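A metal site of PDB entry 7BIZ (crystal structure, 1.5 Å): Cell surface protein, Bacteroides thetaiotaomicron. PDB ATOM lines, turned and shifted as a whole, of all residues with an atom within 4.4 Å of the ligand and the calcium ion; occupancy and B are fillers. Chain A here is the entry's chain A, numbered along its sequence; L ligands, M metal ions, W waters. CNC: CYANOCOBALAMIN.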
ATOM      1  N   GLN A 233     -34.459 -20.642   6.182  1.00  0.00           N
ATOM      2  CA  GLN A 233     -34.758 -19.216   6.306  1.00  0.00           C
ATOM      3  C   GLN A 233     -35.585 -18.661   5.156  1.00  0.00           C
ATOM      4  O   GLN A 233     -36.209 -17.606   5.320  1.00  0.00           O
ATOM      5  CB  GLN A 233     -33.460 -18.440   6.425  1.00  0.00           C
ATOM      6  CG  GLN A 233     -32.669 -18.469   5.115  1.00  0.00           C
ATOM      7  CD  GLN A 233     -31.211 -18.167   5.331  1.00  0.00           C
ATOM      8  OE1 GLN A 233     -30.858 -17.153   5.924  1.00  0.00           O
ATOM      9  NE2 GLN A 233     -30.330 -19.062   4.834  1.00  0.00           N
ATOM     10  N   PHE A 234     -35.599 -19.329   3.998  1.00  0.00           N
ATOM     11  CA  PHE A 234     -36.418 -18.851   2.894  1.00  0.00           C
ATOM     12  C   PHE A 234     -37.784 -19.506   2.853  1.00  0.00           C
ATOM     13  O   PHE A 234     -38.611 -19.129   2.012  1.00  0.00           O
ATOM     14  CB  PHE A 234     -35.666 -19.059   1.581  1.00  0.00           C
ATOM     15  CG  PHE A 234     -34.440 -18.218   1.507  1.00  0.00           C
ATOM     16  CD1 PHE A 234     -34.548 -16.849   1.305  1.00  0.00           C
ATOM     17  CD2 PHE A 234     -33.183 -18.786   1.720  1.00  0.00           C
ATOM     18  CE1 PHE A 234     -33.389 -16.026   1.297  1.00  0.00           C
ATOM     19  CE2 PHE A 234     -32.021 -17.976   1.715  1.00  0.00           C
ATOM     20  CZ  PHE A 234     -32.140 -16.612   1.506  1.00  0.00           C
ATOM     21  N   ILE A 241     -37.594 -10.702  -1.287  1.00  0.00           N
ATOM     22  CA  ILE A 241     -36.503 -11.652  -1.418  1.00  0.00           C
ATOM     23  C   ILE A 241     -36.994 -13.090  -1.336  1.00  0.00           C
ATOM     24  O   ILE A 241     -36.463 -13.978  -2.010  1.00  0.00           O
ATOM     25  CB  ILE A 241     -35.426 -11.343  -0.340  1.00  0.00           C
ATOM     26  CG1 ILE A 241     -34.513 -10.211  -0.835  1.00  0.00           C
ATOM     27  CG2 ILE A 241     -34.639 -12.601   0.054  1.00  0.00           C
ATOM     28  CD1 ILE A 241     -33.389  -9.868   0.141  1.00  0.00           C
ATOM     29  N   HIS A 267     -36.183 -18.308  -7.407  1.00  0.00           N
ATOM     30  CA  HIS A 267     -35.667 -19.415  -6.614  1.00  0.00           C
ATOM     31  C   HIS A 267     -36.758 -20.190  -5.910  1.00  0.00           C
ATOM     32  O   HIS A 267     -37.776 -19.643  -5.479  1.00  0.00           O
ATOM     33  CB  HIS A 267     -34.641 -18.974  -5.552  1.00  0.00           C
ATOM     34  CG  HIS A 267     -35.195 -18.228  -4.371  1.00  0.00           C
ATOM     35  ND1 HIS A 267     -35.855 -18.835  -3.318  1.00  0.00           N
ATOM     36  CD2 HIS A 267     -35.086 -16.918  -4.025  1.00  0.00           C
ATOM     37  CE1 HIS A 267     -36.174 -17.922  -2.413  1.00  0.00           C
ATOM     38  NE2 HIS A 267     -35.705 -16.764  -2.814  1.00  0.00           N
ATOM     39  N   ASN A 299     -27.966 -21.273  -8.236  1.00  0.00           N
ATOM     40  CA  ASN A 299     -27.377 -19.938  -8.154  1.00  0.00           C
ATOM     41  C   ASN A 299     -25.992 -19.993  -7.522  1.00  0.00           C
ATOM     42  O   ASN A 299     -25.570 -19.104  -6.758  1.00  0.00           O
ATOM     43  CB  ASN A 299     -28.308 -18.959  -7.421  1.00  0.00           C
ATOM     44  CG  ASN A 299     -28.657 -19.399  -5.999  1.00  0.00           C
ATOM     45  OD1 ASN A 299     -28.267 -20.489  -5.550  1.00  0.00           O
ATOM     46  ND2 ASN A 299     -29.365 -18.528  -5.270  1.00  0.00           N
ATOM     47  N   PHE A 301     -21.973 -19.861  -6.886  1.00  0.00           N
ATOM     48  CA  PHE A 301     -20.732 -19.189  -7.249  1.00  0.00           C
ATOM     49  C   PHE A 301     -19.680 -19.704  -6.266  1.00  0.00           C
ATOM     50  O   PHE A 301     -20.008 -20.462  -5.334  1.00  0.00           O
ATOM     51  CB  PHE A 301     -20.882 -17.654  -7.262  1.00  0.00           C
ATOM     52  CG  PHE A 301     -21.388 -17.067  -5.981  1.00  0.00           C
ATOM     53  CD1 PHE A 301     -20.498 -16.700  -4.990  1.00  0.00           C
ATOM     54  CD2 PHE A 301     -22.745 -16.865  -5.782  1.00  0.00           C
ATOM     55  CE1 PHE A 301     -20.955 -16.140  -3.783  1.00  0.00           C
ATOM     56  CE2 PHE A 301     -23.221 -16.306  -4.587  1.00  0.00           C
ATOM     57  CZ  PHE A 301     -22.324 -15.956  -3.580  1.00  0.00           C
ATOM     58  N   ASP A 302     -18.414 -19.330  -6.487  1.00  0.00           N
ATOM     59  CA  ASP A 302     -17.342 -19.878  -5.656  1.00  0.00           C
ATOM     60  C   ASP A 302     -17.515 -19.433  -4.200  1.00  0.00           C
ATOM     61  O   ASP A 302     -17.485 -18.239  -3.885  1.00  0.00           O
ATOM     62  CB  ASP A 302     -15.983 -19.433  -6.214  1.00  0.00           C
ATOM     63  CG  ASP A 302     -14.804 -20.169  -5.589  1.00  0.00           C
ATOM     64  OD1 ASP A 302     -14.980 -21.133  -4.809  1.00  0.00           O
ATOM     65  OD2 ASP A 302     -13.647 -19.758  -5.894  1.00  0.00           O
ATOM     66  N   GLY A 303     -17.714 -20.401  -3.291  1.00  0.00           N
ATOM     67  CA  GLY A 303     -18.024 -20.094  -1.914  1.00  0.00           C
ATOM     68  C   GLY A 303     -19.491 -20.270  -1.573  1.00  0.00           C
ATOM     69  O   GLY A 303     -19.855 -20.221  -0.393  1.00  0.00           O
ATOM     70  N   SER A 304     -20.341 -20.485  -2.583  1.00  0.00           N
ATOM     71  CA  SER A 304     -21.776 -20.625  -2.378  1.00  0.00           C
ATOM     72  C   SER A 304     -22.246 -21.900  -3.077  1.00  0.00           C
ATOM     73  O   SER A 304     -23.032 -21.849  -4.014  1.00  0.00           O
ATOM     74  CB  SER A 304     -22.516 -19.404  -2.906  1.00  0.00           C
ATOM     75  OG  SER A 304     -23.872 -19.397  -2.433  1.00  0.00           O
ATOM     76  N   GLU A 306     -24.309 -25.360  -2.427  1.00  0.00           N
ATOM     77  CA  GLU A 306     -25.332 -25.904  -1.527  1.00  0.00           C
ATOM     78  C   GLU A 306     -25.912 -27.127  -2.217  1.00  0.00           C
ATOM     79  O   GLU A 306     -26.987 -27.079  -2.828  1.00  0.00           O
ATOM     80  CB  GLU A 306     -26.415 -24.848  -1.229  1.00  0.00           C
ATOM     81  CG  GLU A 306     -25.870 -23.542  -0.675  1.00  0.00           C
ATOM     82  CD  GLU A 306     -26.963 -22.573  -0.295  1.00  0.00           C
ATOM     83  OE1 GLU A 306     -27.308 -22.494   0.919  1.00  0.00           O
ATOM     84  OE2 GLU A 306     -27.515 -21.910  -1.203  1.00  0.00           O
ATOM     85  N   LEU A 372     -32.896 -16.261  12.082  1.00  0.00           N
ATOM     86  CA  LEU A 372     -32.070 -15.069  11.801  1.00  0.00           C
ATOM     87  C   LEU A 372     -32.963 -13.827  11.709  1.00  0.00           C
ATOM     88  O   LEU A 372     -33.431 -13.429  10.646  1.00  0.00           O
ATOM     89  CB  LEU A 372     -31.264 -15.271  10.511  1.00  0.00           C
ATOM     90  CG  LEU A 372     -30.277 -16.446  10.516  1.00  0.00           C
ATOM     91  CD1 LEU A 372     -29.561 -16.457   9.156  1.00  0.00           C
ATOM     92  CD2 LEU A 372     -29.265 -16.341  11.649  1.00  0.00           C
ATOM     93  N   TYR A 375     -32.501 -10.966   9.150  1.00  0.00           N
ATOM     94  CA  TYR A 375     -32.698 -11.116   7.711  1.00  0.00           C
ATOM     95  C   TYR A 375     -34.046 -11.699   7.309  1.00  0.00           C
ATOM     96  O   TYR A 375     -34.587 -11.309   6.270  1.00  0.00           O
ATOM     97  CB  TYR A 375     -31.586 -11.993   7.099  1.00  0.00           C
ATOM     98  CG  TYR A 375     -30.213 -11.512   7.464  1.00  0.00           C
ATOM     99  CD1 TYR A 375     -29.754 -10.267   7.027  1.00  0.00           C
ATOM    100  CD2 TYR A 375     -29.383 -12.276   8.272  1.00  0.00           C
ATOM    101  CE1 TYR A 375     -28.483  -9.809   7.388  1.00  0.00           C
ATOM    102  CE2 TYR A 375     -28.138 -11.833   8.640  1.00  0.00           C
ATOM    103  CZ  TYR A 375     -27.690 -10.593   8.197  1.00  0.00           C
ATOM    104  OH  TYR A 375     -26.437 -10.153   8.570  1.00  0.00           O
ATOM    105  N   HIS A 376     -34.607 -12.620   8.088  1.00  0.00           N
ATOM    106  CA  HIS A 376     -35.807 -13.338   7.635  1.00  0.00           C
ATOM    107  C   HIS A 376     -36.738 -13.451   8.829  1.00  0.00           C
ATOM    108  O   HIS A 376     -36.522 -14.274   9.722  1.00  0.00           O
ATOM    109  CB  HIS A 376     -35.445 -14.695   7.023  1.00  0.00           C
ATOM    110  CG  HIS A 376     -34.413 -14.581   5.954  1.00  0.00           C
ATOM    111  ND1 HIS A 376     -34.658 -13.970   4.746  1.00  0.00           N
ATOM    112  CD2 HIS A 376     -33.102 -14.950   5.927  1.00  0.00           C
ATOM    113  CE1 HIS A 376     -33.565 -13.987   4.010  1.00  0.00           C
ATOM    114  NE2 HIS A 376     -32.603 -14.574   4.701  1.00  0.00           N
ATOM    115  N   TYR A 410     -15.405 -14.590   7.477  1.00  0.00           N
ATOM    116  CA  TYR A 410     -16.327 -14.915   6.392  1.00  0.00           C
ATOM    117  C   TYR A 410     -16.434 -16.420   6.203  1.00  0.00           C
ATOM    118  O   TYR A 410     -15.502 -17.187   6.469  1.00  0.00           O
ATOM    119  CB  TYR A 410     -15.890 -14.288   5.062  1.00  0.00           C
ATOM    120  CG  TYR A 410     -15.879 -12.779   5.083  1.00  0.00           C
ATOM    121  CD1 TYR A 410     -16.960 -12.060   5.546  1.00  0.00           C
ATOM    122  CD2 TYR A 410     -14.759 -12.065   4.640  1.00  0.00           C
ATOM    123  CE1 TYR A 410     -16.954 -10.681   5.571  1.00  0.00           C
ATOM    124  CE2 TYR A 410     -14.745 -10.690   4.670  1.00  0.00           C
ATOM    125  CZ  TYR A 410     -15.843  -9.998   5.136  1.00  0.00           C
ATOM    126  OH  TYR A 410     -15.847  -8.618   5.178  1.00  0.00           O
ATOM    127  N   TRP A 411     -17.584 -16.819   5.690  1.00  0.00           N
ATOM    128  CA  TRP A 411     -17.917 -18.208   5.479  1.00  0.00           C
ATOM    129  C   TRP A 411     -17.700 -18.616   4.024  1.00  0.00           C
ATOM    130  O   TRP A 411     -17.943 -17.841   3.094  1.00  0.00           O
ATOM    131  CB  TRP A 411     -19.386 -18.454   5.847  1.00  0.00           C
ATOM    132  CG  TRP A 411     -19.615 -18.471   7.320  1.00  0.00           C
ATOM    133  CD1 TRP A 411     -19.899 -17.411   8.131  1.00  0.00           C
ATOM    134  CD2 TRP A 411     -19.569 -19.623   8.172  1.00  0.00           C
ATOM    135  NE1 TRP A 411     -20.053 -17.829   9.439  1.00  0.00           N
ATOM    136  CE2 TRP A 411     -19.856 -19.181   9.483  1.00  0.00           C
ATOM    137  CE3 TRP A 411     -19.310 -20.980   7.946  1.00  0.00           C
ATOM    138  CZ2 TRP A 411     -19.900 -20.061  10.581  1.00  0.00           C
ATOM    139  CZ3 TRP A 411     -19.378 -21.861   9.040  1.00  0.00           C
ATOM    140  CH2 TRP A 411     -19.669 -21.394  10.337  1.00  0.00           C
ATOM    141  N   THR A 434     -20.409 -15.545 -12.423  1.00  0.00           N
ATOM    142  CA  THR A 434     -19.525 -15.989 -11.350  1.00  0.00           C
ATOM    143  C   THR A 434     -19.459 -14.998 -10.214  1.00  0.00           C
ATOM    144  O   THR A 434     -18.832 -15.288  -9.186  1.00  0.00           O
ATOM    145  CB  THR A 434     -18.126 -16.260 -11.898  1.00  0.00           C
ATOM    146  OG1 THR A 434     -17.598 -15.075 -12.501  1.00  0.00           O
ATOM    147  CG2 THR A 434     -18.163 -17.403 -12.922  1.00  0.00           C
ATOM    148  N   VAL A 435     -20.099 -13.842 -10.377  1.00  0.00           N
ATOM    149  CA  VAL A 435     -20.177 -12.871  -9.297  1.00  0.00           C
ATOM    150  C   VAL A 435     -21.320 -13.213  -8.356  1.00  0.00           C
ATOM    151  O   VAL A 435     -21.137 -13.299  -7.137  1.00  0.00           O
ATOM    152  CB  VAL A 435     -20.339 -11.454  -9.869  1.00  0.00           C
ATOM    153  CG1 VAL A 435     -20.577 -10.468  -8.715  1.00  0.00           C
ATOM    154  CG2 VAL A 435     -19.112 -11.071 -10.688  1.00  0.00           C
ATOM    155  N   ASP A 436     -22.527 -13.399  -8.894  1.00  0.00           N
ATOM    156  CA  ASP A 436     -23.685 -13.557  -8.022  1.00  0.00           C
ATOM    157  C   ASP A 436     -24.490 -14.828  -8.282  1.00  0.00           C
ATOM    158  O   ASP A 436     -25.536 -15.016  -7.657  1.00  0.00           O
ATOM    159  CB  ASP A 436     -24.595 -12.320  -8.112  1.00  0.00           C
ATOM    160  CG  ASP A 436     -25.365 -12.192  -9.425  1.00  0.00           C
ATOM    161  OD1 ASP A 436     -25.283 -13.084 -10.293  1.00  0.00           O
ATOM    162  OD2 ASP A 436     -26.037 -11.141  -9.601  1.00  0.00           O
ATOM    163  N   TRP A 477     -24.135 -16.244   9.835  1.00  0.00           N
ATOM    164  CA  TRP A 477     -25.080 -15.259   9.309  1.00  0.00           C
ATOM    165  C   TRP A 477     -25.582 -15.578   7.898  1.00  0.00           C
ATOM    166  O   TRP A 477     -26.493 -14.889   7.424  1.00  0.00           O
ATOM    167  CB  TRP A 477     -24.447 -13.849   9.366  1.00  0.00           C
ATOM    168  CG  TRP A 477     -23.225 -13.595   8.493  1.00  0.00           C
ATOM    169  CD1 TRP A 477     -22.401 -14.523   7.878  1.00  0.00           C
ATOM    170  CD2 TRP A 477     -22.709 -12.312   8.138  1.00  0.00           C
ATOM    171  NE1 TRP A 477     -21.408 -13.872   7.167  1.00  0.00           N
ATOM    172  CE2 TRP A 477     -21.580 -12.510   7.305  1.00  0.00           C
ATOM    173  CE3 TRP A 477     -23.090 -11.009   8.443  1.00  0.00           C
ATOM    174  CZ2 TRP A 477     -20.835 -11.449   6.790  1.00  0.00           C
ATOM    175  CZ3 TRP A 477     -22.373  -9.958   7.922  1.00  0.00           C
ATOM    176  CH2 TRP A 477     -21.233 -10.186   7.110  1.00  0.00           C
ATOM    177  N   LEU A 478     -25.019 -16.577   7.227  1.00  0.00           N
ATOM    178  CA  LEU A 478     -25.603 -17.047   5.975  1.00  0.00           C
ATOM    179  C   LEU A 478     -26.797 -17.953   6.205  1.00  0.00           C
ATOM    180  O   LEU A 478     -27.492 -18.301   5.232  1.00  0.00           O
ATOM    181  CB  LEU A 478     -24.580 -17.813   5.134  1.00  0.00           C
ATOM    182  CG  LEU A 478     -23.252 -17.124   4.849  1.00  0.00           C
ATOM    183  CD1 LEU A 478     -22.442 -17.928   3.789  1.00  0.00           C
ATOM    184  CD2 LEU A 478     -23.519 -15.684   4.374  1.00  0.00           C
ATOM    185  N   GLY A 479     -27.029 -18.401   7.428  1.00  0.00           N
ATOM    186  CA  GLY A 479     -28.155 -19.304   7.618  1.00  0.00           C
ATOM    187  C   GLY A 479     -27.819 -20.713   7.159  1.00  0.00           C
ATOM    188  O   GLY A 479     -26.641 -21.064   6.974  1.00  0.00           O
ATOM    189  N   SER A 482     -28.708 -24.660   1.999  1.00  0.00           N
ATOM    190  CA  SER A 482     -29.988 -25.042   1.378  1.00  0.00           C
ATOM    191  C   SER A 482     -29.894 -24.922  -0.129  1.00  0.00           C
ATOM    192  O   SER A 482     -29.685 -23.823  -0.658  1.00  0.00           O
ATOM    193  CB  SER A 482     -31.122 -24.159   1.891  1.00  0.00           C
ATOM    194  OG  SER A 482     -30.742 -22.783   1.848  1.00  0.00           O
ATOM    195  N   GLU A 484     -30.989 -24.264  -3.779  1.00  0.00           N
ATOM    196  CA  GLU A 484     -32.039 -23.575  -4.534  1.00  0.00           C
ATOM    197  C   GLU A 484     -32.048 -24.059  -5.985  1.00  0.00           C
ATOM    198  O   GLU A 484     -30.981 -24.277  -6.584  1.00  0.00           O
ATOM    199  CB  GLU A 484     -31.863 -22.061  -4.538  1.00  0.00           C
ATOM    200  CG  GLU A 484     -32.432 -21.381  -3.268  1.00  0.00           C
ATOM    201  CD  GLU A 484     -31.452 -21.454  -2.108  1.00  0.00           C
ATOM    202  OE1 GLU A 484     -31.873 -21.523  -0.935  1.00  0.00           O
ATOM    203  OE2 GLU A 484     -30.239 -21.437  -2.353  1.00  0.00           O
HETATM  204 CO   CNC L   1     -23.744 -10.876   0.406  1.00  0.00          CO
HETATM  205  N21 CNC L   1     -22.859 -11.129  -1.236  1.00  0.00           N
HETATM  206  N22 CNC L   1     -22.101 -10.719   1.287  1.00  0.00           N
HETATM  207  N23 CNC L   1     -24.743 -11.380   1.902  1.00  0.00           N
HETATM  208  N24 CNC L   1     -25.276 -10.779  -0.717  1.00  0.00           N
HETATM  209  C1  CNC L   1     -23.637 -10.861  -2.408  1.00  0.00           C
HETATM  210  C20 CNC L   1     -23.864 -12.391  -2.613  1.00  0.00           C
HETATM  211  C2  CNC L   1     -22.794 -10.533  -3.636  1.00  0.00           C
HETATM  212  C25 CNC L   1     -22.967 -11.401  -4.907  1.00  0.00           C
HETATM  213  C26 CNC L   1     -23.244  -9.103  -3.907  1.00  0.00           C
HETATM  214  C27 CNC L   1     -22.294  -8.272  -4.788  1.00  0.00           C
HETATM  215  O28 CNC L   1     -22.378  -8.345  -6.004  1.00  0.00           O
HETATM  216  N29 CNC L   1     -21.401  -7.469  -4.204  1.00  0.00           N
HETATM  217  C3  CNC L   1     -21.376 -10.527  -2.986  1.00  0.00           C
HETATM  218  C30 CNC L   1     -20.458 -11.805  -3.269  1.00  0.00           C
HETATM  219  C31 CNC L   1     -19.546 -11.649  -4.537  1.00  0.00           C
HETATM  220  C32 CNC L   1     -18.606 -12.842  -4.632  1.00  0.00           C
HETATM  221  O34 CNC L   1     -18.777 -13.733  -5.496  1.00  0.00           O
HETATM  222  N33 CNC L   1     -17.581 -12.936  -3.789  1.00  0.00           N
HETATM  223  C4  CNC L   1     -21.704 -10.527  -1.507  1.00  0.00           C
HETATM  224  C5  CNC L   1     -20.668 -10.156  -0.554  1.00  0.00           C
HETATM  225  C35 CNC L   1     -19.517  -9.277  -1.189  1.00  0.00           C
HETATM  226  C6  CNC L   1     -20.926 -10.151   0.804  1.00  0.00           C
HETATM  227  C7  CNC L   1     -19.901  -9.903   1.912  1.00  0.00           C
HETATM  228  C36 CNC L   1     -18.377 -10.261   1.677  1.00  0.00           C
HETATM  229  C37 CNC L   1     -20.145  -8.418   2.294  1.00  0.00           C
HETATM  230  C38 CNC L   1     -19.292  -7.972   3.517  1.00  0.00           C
HETATM  231  O39 CNC L   1     -18.247  -7.283   3.301  1.00  0.00           O
HETATM  232  N40 CNC L   1     -19.658  -8.247   4.740  1.00  0.00           N
HETATM  233  C8  CNC L   1     -20.510 -10.812   3.065  1.00  0.00           C
HETATM  234  C41 CNC L   1     -19.798 -12.206   3.015  1.00  0.00           C
HETATM  235  C42 CNC L   1     -20.650 -13.330   3.680  1.00  0.00           C
HETATM  236  C43 CNC L   1     -19.825 -14.540   3.976  1.00  0.00           C
HETATM  237  O44 CNC L   1     -19.506 -14.825   5.152  1.00  0.00           O
HETATM  238  N45 CNC L   1     -19.402 -15.308   2.950  1.00  0.00           N
HETATM  239  C9  CNC L   1     -21.933 -10.878   2.571  1.00  0.00           C
HETATM  240  C10 CNC L   1     -22.937 -11.039   3.542  1.00  0.00           C
HETATM  241  C11 CNC L   1     -24.295 -11.087   3.160  1.00  0.00           C
HETATM  242  C12 CNC L   1     -25.349 -11.069   4.267  1.00  0.00           C
HETATM  243  C46 CNC L   1     -24.991 -12.104   5.407  1.00  0.00           C
HETATM  244  C47 CNC L   1     -25.470  -9.660   4.912  1.00  0.00           C
HETATM  245  C13 CNC L   1     -26.641 -11.350   3.430  1.00  0.00           C
HETATM  246  C48 CNC L   1     -27.186 -12.834   3.636  1.00  0.00           C
HETATM  247  C49 CNC L   1     -28.154 -12.937   4.853  1.00  0.00           C
HETATM  248  C50 CNC L   1     -29.024 -14.218   4.837  1.00  0.00           C
HETATM  249  O51 CNC L   1     -28.834 -15.146   5.708  1.00  0.00           O
HETATM  250  N52 CNC L   1     -29.939 -14.318   3.934  1.00  0.00           N
HETATM  251  C14 CNC L   1     -26.078 -11.107   2.027  1.00  0.00           C
HETATM  252  C15 CNC L   1     -27.004 -11.044   0.974  1.00  0.00           C
HETATM  253  C53 CNC L   1     -28.513 -10.948   1.296  1.00  0.00           C
HETATM  254  C16 CNC L   1     -26.483 -11.045  -0.381  1.00  0.00           C
HETATM  255  C17 CNC L   1     -27.446 -10.752  -1.590  1.00  0.00           C
HETATM  256  C54 CNC L   1     -27.888  -9.244  -1.718  1.00  0.00           C
HETATM  257  C55 CNC L   1     -28.651 -11.655  -1.809  1.00  0.00           C
HETATM  258  C56 CNC L   1     -28.337 -13.153  -1.526  1.00  0.00           C
HETATM  259  C57 CNC L   1     -29.652 -13.928  -1.561  1.00  0.00           C
HETATM  260  O58 CNC L   1     -30.568 -13.598  -0.826  1.00  0.00           O
HETATM  261  N59 CNC L   1     -29.770 -14.933  -2.397  1.00  0.00           N
HETATM  262  C18 CNC L   1     -26.454 -11.090  -2.717  1.00  0.00           C
HETATM  263  C60 CNC L   1     -26.591 -10.318  -4.079  1.00  0.00           C
HETATM  264  C61 CNC L   1     -27.826 -10.733  -4.848  1.00  0.00           C
HETATM  265  O63 CNC L   1     -28.687  -9.904  -5.132  1.00  0.00           O
HETATM  266  N62 CNC L   1     -27.954 -12.016  -5.184  1.00  0.00           N
HETATM  267  C19 CNC L   1     -25.111 -10.699  -2.163  1.00  0.00           C
HETATM  268  C1P CNC L   1     -31.065 -15.672  -2.433  1.00  0.00           C
HETATM  269  C2P CNC L   1     -30.945 -17.037  -1.759  1.00  0.00           C
HETATM  270  C3P CNC L   1     -32.274 -17.769  -1.819  1.00  0.00           C
HETATM  271  O3  CNC L   1     -29.932 -17.835  -2.416  1.00  0.00           O
HETATM  272  O4  CNC L   1     -29.214 -19.244  -0.402  1.00  0.00           O
HETATM  273  O5  CNC L   1     -27.883 -19.280  -2.556  1.00  0.00           O
HETATM  274  P   CNC L   1     -28.739 -18.493  -1.595  1.00  0.00           P
HETATM  275  O2  CNC L   1     -27.950 -17.155  -1.028  1.00  0.00           O
HETATM  276  C3R CNC L   1     -26.946 -17.331  -0.062  1.00  0.00           C
HETATM  277  C2R CNC L   1     -25.614 -16.718  -0.469  1.00  0.00           C
HETATM  278  O7R CNC L   1     -25.876 -15.513  -1.154  1.00  0.00           O
HETATM  279  C1R CNC L   1     -24.928 -16.501   0.923  1.00  0.00           C
HETATM  280  O6R CNC L   1     -25.972 -16.191   1.792  1.00  0.00           O
HETATM  281  C4R CNC L   1     -27.248 -16.366   1.113  1.00  0.00           C
HETATM  282  C5R CNC L   1     -28.290 -16.921   2.108  1.00  0.00           C
HETATM  283  O8R CNC L   1     -27.789 -18.204   2.593  1.00  0.00           O
HETATM  284  N1B CNC L   1     -24.094 -15.317   0.778  1.00  0.00           N
HETATM  285  C8B CNC L   1     -22.761 -15.321   0.398  1.00  0.00           C
HETATM  286  C2B CNC L   1     -24.541 -14.080   0.878  1.00  0.00           C
HETATM  287  N3B CNC L   1     -23.522 -13.258   0.590  1.00  0.00           N
HETATM  288  C9B CNC L   1     -22.387 -13.986   0.293  1.00  0.00           C
HETATM  289  C4B CNC L   1     -21.075 -13.648  -0.063  1.00  0.00           C
HETATM  290  C5B CNC L   1     -20.134 -14.630  -0.289  1.00  0.00           C
HETATM  291  C5M CNC L   1     -18.704 -14.270  -0.666  1.00  0.00           C
HETATM  292  C6B CNC L   1     -20.503 -16.024  -0.178  1.00  0.00           C
HETATM  293  C6M CNC L   1     -19.503 -17.069  -0.422  1.00  0.00           C
HETATM  294  C7B CNC L   1     -21.826 -16.344   0.170  1.00  0.00           C
HETATM  295  N1A CNC L   1     -24.144  -7.704   0.511  1.00  0.00           N
HETATM  296  C1A CNC L   1     -23.989  -8.842   0.491  1.00  0.00           C
HETATM  297 CA    CA M   1     -29.589 -21.524   0.082  1.00  0.00          CA
HETATM  298  O   HOH W   1     -25.712 -21.361  -4.245  1.00  0.00           O
HETATM  299  O   HOH W   2     -26.022 -13.777  -5.201  1.00  0.00           O
HETATM  300  O   HOH W   3     -18.288  -7.727   6.970  1.00  0.00           O
HETATM  301  O   HOH W   4     -28.340  -6.978  -4.590  1.00  0.00           O
HETATM  302  O   HOH W   5     -16.904 -16.086  -5.669  1.00  0.00           O
HETATM  303  O   HOH W   6     -31.290 -13.067   1.880  1.00  0.00           O
HETATM  304  O   HOH W   7     -16.490 -11.006  -2.373  1.00  0.00           O
HETATM  305  O   HOH W   8     -31.497 -10.650   2.906  1.00  0.00           O
HETATM  306  O   HOH W   9     -29.982 -13.501  -5.860  1.00  0.00           O
HETATM  307  O   HOH W  10     -27.128 -15.615  -3.643  1.00  0.00           O
HETATM  308  O   HOH W  11     -29.312 -20.578   2.273  1.00  0.00           O
HETATM  309  O   HOH W  12     -32.121 -12.082  -2.883  1.00  0.00           O
HETATM  310  O   HOH W  13     -26.090 -20.359   1.975  1.00  0.00           O
HETATM  311  O   HOH W  14     -19.428  -7.610  -6.843  1.00  0.00           O
HETATM  312  O   HOH W  15     -25.915 -18.271  -4.007  1.00  0.00           O
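The calcium ion is bound by an oxygen (O4) of the ligand (2.4 Å), water W11 (2.4 Å), the backbone carbonyl oxygen (O) of Ser 482 (2.4 Å), the side-chain hydroxyl (OG) of Ser 482 (2.5 Å), the side-chain carboxylate (OE2) of Glu 306 (2.5 Å), the side-chain carboxylate (OE1) of Glu 484 (2.5 Å), the side-chain carboxylate (OE2) of Glu 484 (2.5 Å) and the side-chain carboxylate (OE1) of Glu 306 (2.6 Å).
The calcium ion has eight donor atoms within binding distance.
Of the 23 residues printed, 3 come within 4 Å of the calcium ion.
Water W11 lies within hydrogen-bond range of O8R of the ligand and NE2 of Gln 233.
Water W2 bridges a nitrogen (N62) of the ligand (2.6 Å) and the backbone carbonyl oxygen (O) of Asp 436 (2.8 Å).
Water W15 lies within hydrogen-bond range of an oxygen (O5) of the ligand (2.6 Å), the side-chain hydroxyl (OG) of Ser 304 (2.8 Å) and the backbone carbonyl oxygen (O) of Asn 299 (2.9 Å).
Water W3 bridges N40 of the ligand (2.7 Å) and OH of Tyr 410 (3.2 Å).
Water W6 lies within hydrogen-bond range of a nitrogen (N52) of the ligand (2.8 Å) and a ring nitrogen (NE2) of His 376 (3.5 Å).
Water W5 lies within hydrogen-bond range of the backbone carbonyl oxygen of Asp 302 (2.9 Å) and an oxygen (O34) of the ligand (3.0 Å).
N52 of the ligand lies within hydrogen-bond range of NE2 of His 376.
The side-chain amide oxygen (OE1) of Gln 233 lies close to an oxygen (O51) of the ligand.
The side-chain amide nitrogen (ND2) of Asn 299 sits at hydrogen-bond distance from an oxygen (O3) of the ligand (3.0 Å).
OH of Tyr 410 is in hydrogen-bond range of O39 of the ligand, 3.3 Å away.
O of Trp 411 lies within hydrogen-bond range of N45 of the ligand, at 2.9 Å.
An oxygen (O8R) of the ligand lies within hydrogen-bond range of the backbone carbonyl oxygen (O) of Leu 478.
The indole nitrogen of Trp 477 is in hydrogen-bond range of an oxygen (O44) of the ligand (2.9 Å).
An oxygen (O44) of the ligand lies within hydrogen-bond range of the backbone NH (N) of Trp 411, at 2.8 Å.
The side-chain amide oxygen (OE1) of Gln 233 lies close to a ring nitrogen (NE2) of His 376, 3.3 Å away.
The side-chain amide nitrogen (NE2) of Gln 233 sits at hydrogen-bond distance from the backbone carbonyl oxygen (O) of Leu 478, at 3.0 Å.
The backbone carbonyl oxygen (O) of Ile 241 sits at hydrogen-bond distance from a ring nitrogen (NE2) of His 267, at 3.0 Å.
O34 of the ligand sits close to O of Val 435 (2.9 Å).
CZ of Phe 234 touches C2P of the ligand (3.5 Å).
His 267 touches the ligand.
Phe 301 touches the ligand.
Gly 303 touches the ligand (O to C6M, 3.2 Å).
Ser 304 touches the ligand (OG to C2R, 3.8 Å).
Leu 372 touches the ligand.
CG of Tyr 375 touches C49 of the ligand (3.6 Å).
CB of Asp 436 touches C25 of the ligand, 3.7 Å away.
Hydrophobic or aromatic side chains within 4 Å of the ligand: Phe 234, His 267, Phe 301, Leu 372, Tyr 375, His 376, Tyr 410, Trp 411, Val 435, Trp 477 and Leu 478.
Within 4 Å of the ligand: Gln 233, Phe 234, His 267, Asn 299, Phe 301, Gly 303, Ser 304, Glu 306, Leu 372, Tyr 375, His 376, Tyr 410, Trp 411, Val 435, Asp 436, Trp 477, Leu 478 and Glu 484.
The nearest printed residue that does not touch the ligand is Thr 434 (4.005 Å).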
